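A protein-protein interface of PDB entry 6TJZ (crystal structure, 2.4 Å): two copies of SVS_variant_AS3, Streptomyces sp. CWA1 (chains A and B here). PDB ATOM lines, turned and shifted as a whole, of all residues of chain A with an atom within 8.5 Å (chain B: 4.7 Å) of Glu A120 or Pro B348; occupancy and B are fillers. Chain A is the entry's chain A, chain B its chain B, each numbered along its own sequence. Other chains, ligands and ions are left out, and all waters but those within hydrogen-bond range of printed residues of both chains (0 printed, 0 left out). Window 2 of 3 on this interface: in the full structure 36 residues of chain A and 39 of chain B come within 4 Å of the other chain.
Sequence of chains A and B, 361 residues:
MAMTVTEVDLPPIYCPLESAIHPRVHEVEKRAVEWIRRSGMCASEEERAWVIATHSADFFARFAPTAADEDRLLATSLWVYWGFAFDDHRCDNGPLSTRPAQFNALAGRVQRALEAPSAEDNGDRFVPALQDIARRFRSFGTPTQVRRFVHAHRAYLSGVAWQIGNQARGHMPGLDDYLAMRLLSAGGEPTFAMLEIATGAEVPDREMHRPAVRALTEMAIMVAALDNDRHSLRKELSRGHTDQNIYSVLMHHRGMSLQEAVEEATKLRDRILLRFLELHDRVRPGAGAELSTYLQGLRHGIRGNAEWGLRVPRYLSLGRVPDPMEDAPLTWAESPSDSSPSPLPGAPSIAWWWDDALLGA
The side-chain hydroxyl of Ser A118 is in hydrogen-bond range of the backbone NH of Trp B352 (3.2 Å). The side-chain hydroxyl (OG) of Ser A118 is in hydrogen-bond range of the backbone carbonyl oxygen (O) of Pro B348 (2.4 Å). O of Ser B349 sits at hydrogen-bond distance from NH2 of Arg A112 (3.0 Å).
O of Ala A116 is in hydrogen-bond range of NE2 of Gln A131, at 3.5 Å. OD1 of Asp B176 lies within hydrogen-bond range of N of Ser B349 (2.8 Å).
Among the printed residues, merely in contact across the chains: Arg A112 with Ile B350 (3.96 Å), Arg A112 with Trp B352 (3.5 Å), Ala A116 with Ser B349 (3.3 Å), Ala A116 with Trp B352 (3.4 Å), Ser A118 with Ser B349 (3.8 Å), Ser A118 with Ala B351 (3.6 Å) and Glu A120 with Pro B348 (3.8 Å).
Of chain B, only Pro B348 comes within 4 Å of Glu A120. Pro B348 touches two residues of chain A. No residue of chain A comes within 4 Å of Ala B347. Of the printed residues of chain B, Arg A112 touches Ser B349, Ile B350 and Trp B352. Printed residues of chain A within 4 Å of Ile B350: Arg A112. Of the printed residues of chain B, Ala A116 touches Ser B349 (3.3 Å) and Trp B352 (3.4 Å). Asp A121 touches none of the printed residues of chain B. The nearest printed residue of chain B that does not touch Ala A116 is Ile B350 (5.5 Å).
Hydrophobic or aromatic side chains of chain B that line the printed part of chain A: Pro B348, Ile B350, Ala B351 and Trp B352. Of the 16 printed residues of chain A, 4 touch a printed residue of chain B. Hydrophobic or aromatic side chains of chain A within 4 Å of the printed part of chain B: Ala A116. Among the printed residues, 10 pairs touch across the chains.
No position is printed for both chains. Of the 10 pairs that touch across the chains among the printed residues, none has its exchanged pair printed and touching as well.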
ATOM      1  N   ARG A 109      -4.777   4.843 -12.794  1.00  0.00           N
ATOM      2  CA  ARG A 109      -4.491   3.397 -12.560  1.00  0.00           C
ATOM      3  C   ARG A 109      -5.387   2.576 -13.493  1.00  0.00           C
ATOM      4  O   ARG A 109      -4.869   1.656 -14.138  1.00  0.00           O
ATOM      5  CB  ARG A 109      -4.651   2.976 -11.085  1.00  0.00           C
ATOM      6  CG  ARG A 109      -3.610   3.573 -10.139  1.00  0.00           C
ATOM      7  CD  ARG A 109      -3.507   2.971  -8.738  1.00  0.00           C
ATOM      8  NE  ARG A 109      -4.824   2.679  -8.207  1.00  0.00           N
ATOM      9  CZ  ARG A 109      -5.587   3.511  -7.493  1.00  0.00           C
ATOM     10  NH1 ARG A 109      -5.152   4.718  -7.160  1.00  0.00           N
ATOM     11  NH2 ARG A 109      -6.795   3.117  -7.109  1.00  0.00           N
ATOM     12  N   VAL A 110      -6.672   2.922 -13.592  1.00  0.00           N
ATOM     13  CA  VAL A 110      -7.637   2.130 -14.397  1.00  0.00           C
ATOM     14  C   VAL A 110      -7.251   2.290 -15.868  1.00  0.00           C
ATOM     15  O   VAL A 110      -7.175   1.279 -16.584  1.00  0.00           O
ATOM     16  CB  VAL A 110      -9.090   2.518 -14.079  1.00  0.00           C
ATOM     17  CG1 VAL A 110     -10.047   2.016 -15.129  1.00  0.00           C
ATOM     18  CG2 VAL A 110      -9.493   1.975 -12.719  1.00  0.00           C
ATOM     19  N   ARG A 112      -4.286   2.962 -17.111  1.00  0.00           N
ATOM     20  CA  ARG A 112      -2.976   2.295 -17.343  1.00  0.00           C
ATOM     21  C   ARG A 112      -3.195   0.781 -17.493  1.00  0.00           C
ATOM     22  O   ARG A 112      -2.610   0.164 -18.421  1.00  0.00           O
ATOM     23  CB  ARG A 112      -2.005   2.621 -16.207  1.00  0.00           C
ATOM     24  CG  ARG A 112      -0.583   2.146 -16.470  1.00  0.00           C
ATOM     25  CD  ARG A 112      -0.019   2.675 -17.771  1.00  0.00           C
ATOM     26  NE  ARG A 112       1.283   2.106 -18.088  1.00  0.00           N
ATOM     27  CZ  ARG A 112       1.863   2.139 -19.287  1.00  0.00           C
ATOM     28  NH1 ARG A 112       1.259   2.708 -20.319  1.00  0.00           N
ATOM     29  NH2 ARG A 112       3.050   1.581 -19.456  1.00  0.00           N
ATOM     30  N   ALA A 113      -4.057   0.218 -16.649  1.00  0.00           N
ATOM     31  CA  ALA A 113      -4.462  -1.204 -16.690  1.00  0.00           C
ATOM     32  C   ALA A 113      -5.039  -1.560 -18.063  1.00  0.00           C
ATOM     33  O   ALA A 113      -4.867  -2.721 -18.495  1.00  0.00           O
ATOM     34  CB  ALA A 113      -5.437  -1.471 -15.581  1.00  0.00           C
ATOM     35  N   ALA A 116      -1.887  -1.406 -20.605  1.00  0.00           N
ATOM     36  CA  ALA A 116      -0.731  -2.218 -20.161  1.00  0.00           C
ATOM     37  C   ALA A 116      -1.231  -3.537 -19.575  1.00  0.00           C
ATOM     38  O   ALA A 116      -1.639  -3.570 -18.418  1.00  0.00           O
ATOM     39  CB  ALA A 116       0.067  -1.415 -19.164  1.00  0.00           C
ATOM     40  N   PRO A 117      -1.260  -4.643 -20.356  1.00  0.00           N
ATOM     41  CA  PRO A 117      -1.750  -5.939 -19.871  1.00  0.00           C
ATOM     42  C   PRO A 117      -1.003  -6.489 -18.647  1.00  0.00           C
ATOM     43  O   PRO A 117      -1.567  -7.334 -17.969  1.00  0.00           O
ATOM     44  CB  PRO A 117      -1.522  -6.923 -21.037  1.00  0.00           C
ATOM     45  CG  PRO A 117      -1.385  -6.040 -22.263  1.00  0.00           C
ATOM     46  CD  PRO A 117      -0.818  -4.721 -21.764  1.00  0.00           C
ATOM     47  N   SER A 118       0.215  -5.996 -18.391  1.00  0.00           N
ATOM     48  CA  SER A 118       1.104  -6.432 -17.278  1.00  0.00           C
ATOM     49  C   SER A 118       0.767  -5.703 -15.963  1.00  0.00           C
ATOM     50  O   SER A 118       1.310  -6.093 -14.916  1.00  0.00           O
ATOM     51  CB  SER A 118       2.545  -6.242 -17.664  1.00  0.00           C
ATOM     52  OG  SER A 118       2.870  -4.859 -17.839  1.00  0.00           O
ATOM     53  N   ALA A 119      -0.105  -4.696 -15.991  1.00  0.00           N
ATOM     54  CA  ALA A 119      -0.524  -3.915 -14.804  1.00  0.00           C
ATOM     55  C   ALA A 119      -1.243  -4.834 -13.811  1.00  0.00           C
ATOM     56  O   ALA A 119      -1.873  -5.815 -14.259  1.00  0.00           O
ATOM     57  CB  ALA A 119      -1.401  -2.757 -15.223  1.00  0.00           C
ATOM     58  N   GLU A 120      -1.132  -4.518 -12.519  1.00  0.00           N
ATOM     59  CA  GLU A 120      -1.734  -5.281 -11.392  1.00  0.00           C
ATOM     60  C   GLU A 120      -2.907  -4.476 -10.823  1.00  0.00           C
ATOM     61  O   GLU A 120      -2.926  -3.249 -11.007  1.00  0.00           O
ATOM     62  CB  GLU A 120      -0.681  -5.565 -10.321  1.00  0.00           C
ATOM     63  CG  GLU A 120       0.043  -6.888 -10.520  1.00  0.00           C
ATOM     64  CD  GLU A 120       1.252  -7.070  -9.611  1.00  0.00           C
ATOM     65  OE1 GLU A 120       1.320  -6.396  -8.551  1.00  0.00           O
ATOM     66  OE2 GLU A 120       2.139  -7.869  -9.973  1.00  0.00           O
ATOM     67  N   ASP A 121      -3.844  -5.130 -10.176  1.00  0.00           N
ATOM     68  CA  ASP A 121      -5.027  -4.451  -9.719  1.00  0.00           C
ATOM     69  C   ASP A 121      -4.976  -3.580  -8.499  1.00  0.00           C
ATOM     70  O   ASP A 121      -5.812  -2.708  -8.386  1.00  0.00           O
ATOM     71  CB  ASP A 121      -6.140  -5.457  -9.532  1.00  0.00           C
ATOM     72  CG  ASP A 121      -5.846  -6.434  -8.465  1.00  0.00           C
ATOM     73  OD1 ASP A 121      -6.295  -7.568  -8.572  1.00  0.00           O
ATOM     74  OD2 ASP A 121      -5.166  -6.084  -7.508  1.00  0.00           O
ATOM     75  N   ASN A 122      -4.008  -3.800  -7.616  1.00  0.00           N
ATOM     76  CA  ASN A 122      -3.894  -3.088  -6.349  1.00  0.00           C
ATOM     77  C   ASN A 122      -5.198  -3.213  -5.616  1.00  0.00           C
ATOM     78  O   ASN A 122      -5.684  -2.270  -5.042  1.00  0.00           O
ATOM     79  CB  ASN A 122      -3.499  -1.614  -6.475  1.00  0.00           C
ATOM     80  CG  ASN A 122      -2.443  -1.388  -7.517  1.00  0.00           C
ATOM     81  OD1 ASN A 122      -1.608  -2.252  -7.754  1.00  0.00           O
ATOM     82  ND2 ASN A 122      -2.469  -0.226  -8.145  1.00  0.00           N
ATOM     83  N   GLY A 123      -5.768  -4.398  -5.669  1.00  0.00           N
ATOM     84  CA  GLY A 123      -7.034  -4.716  -4.975  1.00  0.00           C
ATOM     85  C   GLY A 123      -8.240  -3.918  -5.468  1.00  0.00           C
ATOM     86  O   GLY A 123      -9.262  -3.934  -4.751  1.00  0.00           O
ATOM     87  N   ASP A 124      -8.170  -3.250  -6.629  1.00  0.00           N
ATOM     88  CA  ASP A 124      -9.368  -2.616  -7.249  1.00  0.00           C
ATOM     89  C   ASP A 124     -10.099  -3.666  -8.098  1.00  0.00           C
ATOM     90  O   ASP A 124      -9.482  -4.144  -9.058  1.00  0.00           O
ATOM     91  CB  ASP A 124      -9.036  -1.379  -8.083  1.00  0.00           C
ATOM     92  CG  ASP A 124     -10.302  -0.754  -8.655  1.00  0.00           C
ATOM     93  OD1 ASP A 124     -11.346  -1.456  -8.692  1.00  0.00           O
ATOM     94  OD2 ASP A 124     -10.260   0.425  -9.026  1.00  0.00           O
ATOM     95  N   VAL A 127     -10.533  -3.452 -12.177  1.00  0.00           N
ATOM     96  CA  VAL A 127      -9.327  -3.493 -13.057  1.00  0.00           C
ATOM     97  C   VAL A 127      -9.255  -4.854 -13.750  1.00  0.00           C
ATOM     98  O   VAL A 127      -9.204  -4.875 -14.978  1.00  0.00           O
ATOM     99  CB  VAL A 127      -8.043  -3.086 -12.310  1.00  0.00           C
ATOM    100  CG1 VAL A 127      -6.778  -3.619 -12.972  1.00  0.00           C
ATOM    101  CG2 VAL A 127      -7.970  -1.574 -12.175  1.00  0.00           C
ATOM    102  N   PRO A 128      -9.251  -6.016 -13.045  1.00  0.00           N
ATOM    103  CA  PRO A 128      -9.177  -7.314 -13.722  1.00  0.00           C
ATOM    104  C   PRO A 128     -10.302  -7.501 -14.751  1.00  0.00           C
ATOM    105  O   PRO A 128     -10.043  -7.979 -15.835  1.00  0.00           O
ATOM    106  CB  PRO A 128      -9.261  -8.347 -12.582  1.00  0.00           C
ATOM    107  CG  PRO A 128      -8.722  -7.581 -11.378  1.00  0.00           C
ATOM    108  CD  PRO A 128      -9.237  -6.167 -11.579  1.00  0.00           C
ATOM    109  N   GLN A 131      -9.341  -5.458 -17.774  1.00  0.00           N
ATOM    110  CA  GLN A 131      -8.173  -6.101 -18.441  1.00  0.00           C
ATOM    111  C   GLN A 131      -8.637  -7.271 -19.291  1.00  0.00           C
ATOM    112  O   GLN A 131      -8.029  -7.464 -20.355  1.00  0.00           O
ATOM    113  CB  GLN A 131      -7.121  -6.572 -17.441  1.00  0.00           C
ATOM    114  CG  GLN A 131      -6.394  -5.389 -16.836  1.00  0.00           C
ATOM    115  CD  GLN A 131      -5.147  -5.799 -16.112  1.00  0.00           C
ATOM    116  OE1 GLN A 131      -5.232  -6.498 -15.115  1.00  0.00           O
ATOM    117  NE2 GLN A 131      -4.003  -5.322 -16.592  1.00  0.00           N
ATOM    118  N   ASP B 176       5.604   1.769  -9.226  1.00  0.00           N
ATOM    119  CA  ASP B 176       4.741   1.436 -10.383  1.00  0.00           C
ATOM    120  C   ASP B 176       3.831   2.634 -10.712  1.00  0.00           C
ATOM    121  O   ASP B 176       3.748   3.012 -11.894  1.00  0.00           O
ATOM    122  CB  ASP B 176       3.910   0.188 -10.109  1.00  0.00           C
ATOM    123  CG  ASP B 176       3.123  -0.256 -11.332  1.00  0.00           C
ATOM    124  OD1 ASP B 176       3.768  -0.535 -12.391  1.00  0.00           O
ATOM    125  OD2 ASP B 176       1.889  -0.294 -11.224  1.00  0.00           O
ATOM    126  N   GLY B 346       8.784  -4.578  -9.324  1.00  0.00           N
ATOM    127  CA  GLY B 346       8.069  -3.509  -8.598  1.00  0.00           C
ATOM    128  C   GLY B 346       7.414  -2.487  -9.522  1.00  0.00           C
ATOM    129  O   GLY B 346       6.879  -1.496  -8.977  1.00  0.00           O
ATOM    130  N   ALA B 347       7.443  -2.703 -10.851  1.00  0.00           N
ATOM    131  CA  ALA B 347       6.844  -1.815 -11.886  1.00  0.00           C
ATOM    132  C   ALA B 347       6.149  -2.667 -12.939  1.00  0.00           C
ATOM    133  O   ALA B 347       6.495  -2.648 -14.123  1.00  0.00           O
ATOM    134  CB  ALA B 347       7.896  -0.929 -12.500  1.00  0.00           C
ATOM    135  N   PRO B 348       5.147  -3.464 -12.519  1.00  0.00           N
ATOM    136  CA  PRO B 348       4.467  -4.361 -13.446  1.00  0.00           C
ATOM    137  C   PRO B 348       3.829  -3.606 -14.629  1.00  0.00           C
ATOM    138  O   PRO B 348       3.879  -4.155 -15.734  1.00  0.00           O
ATOM    139  CB  PRO B 348       3.460  -5.117 -12.561  1.00  0.00           C
ATOM    140  CG  PRO B 348       3.334  -4.295 -11.280  1.00  0.00           C
ATOM    141  CD  PRO B 348       4.638  -3.540 -11.140  1.00  0.00           C
ATOM    142  N   SER B 349       3.355  -2.362 -14.427  1.00  0.00           N
ATOM    143  CA  SER B 349       2.656  -1.562 -15.474  1.00  0.00           C
ATOM    144  C   SER B 349       3.557  -1.284 -16.685  1.00  0.00           C
ATOM    145  O   SER B 349       2.994  -0.874 -17.712  1.00  0.00           O
ATOM    146  CB  SER B 349       2.106  -0.262 -14.949  1.00  0.00           C
ATOM    147  OG  SER B 349       3.038   0.794 -15.165  1.00  0.00           O
ATOM    148  N   ILE B 350       4.883  -1.438 -16.579  1.00  0.00           N
ATOM    149  CA  ILE B 350       5.820  -1.185 -17.714  1.00  0.00           C
ATOM    150  C   ILE B 350       6.486  -2.498 -18.159  1.00  0.00           C
ATOM    151  O   ILE B 350       7.216  -2.461 -19.165  1.00  0.00           O
ATOM    152  CB  ILE B 350       6.854  -0.078 -17.378  1.00  0.00           C
ATOM    153  CG1 ILE B 350       7.848  -0.512 -16.299  1.00  0.00           C
ATOM    154  CG2 ILE B 350       6.157   1.232 -17.022  1.00  0.00           C
ATOM    155  CD1 ILE B 350       9.025   0.431 -16.122  1.00  0.00           C
ATOM    156  N   ALA B 351       6.211  -3.619 -17.491  1.00  0.00           N
ATOM    157  CA  ALA B 351       6.833  -4.944 -17.767  1.00  0.00           C
ATOM    158  C   ALA B 351       6.567  -5.390 -19.222  1.00  0.00           C
ATOM    159  O   ALA B 351       7.434  -6.057 -19.824  1.00  0.00           O
ATOM    160  CB  ALA B 351       6.342  -5.964 -16.761  1.00  0.00           C
ATOM    161  N   TRP B 352       5.429  -5.017 -19.805  1.00  0.00           N
ATOM    162  CA  TRP B 352       5.069  -5.482 -21.165  1.00  0.00           C
ATOM    163  C   TRP B 352       6.053  -4.921 -22.182  1.00  0.00           C
ATOM    164  O   TRP B 352       6.076  -5.447 -23.306  1.00  0.00           O
ATOM    165  CB  TRP B 352       3.638  -5.104 -21.532  1.00  0.00           C
ATOM    166  CG  TRP B 352       3.375  -3.638 -21.654  1.00  0.00           C
ATOM    167  CD1 TRP B 352       3.058  -2.768 -20.652  1.00  0.00           C
ATOM    168  CD2 TRP B 352       3.364  -2.873 -22.862  1.00  0.00           C
ATOM    169  NE1 TRP B 352       2.838  -1.518 -21.155  1.00  0.00           N
ATOM    170  CE2 TRP B 352       3.016  -1.551 -22.509  1.00  0.00           C
ATOM    171  CE3 TRP B 352       3.560  -3.188 -24.203  1.00  0.00           C
ATOM    172  CZ2 TRP B 352       2.897  -0.536 -23.449  1.00  0.00           C
ATOM    173  CZ3 TRP B 352       3.450  -2.182 -25.139  1.00  0.00           C
ATOM    174  CH2 TRP B 352       3.131  -0.875 -24.767  1.00  0.00           C
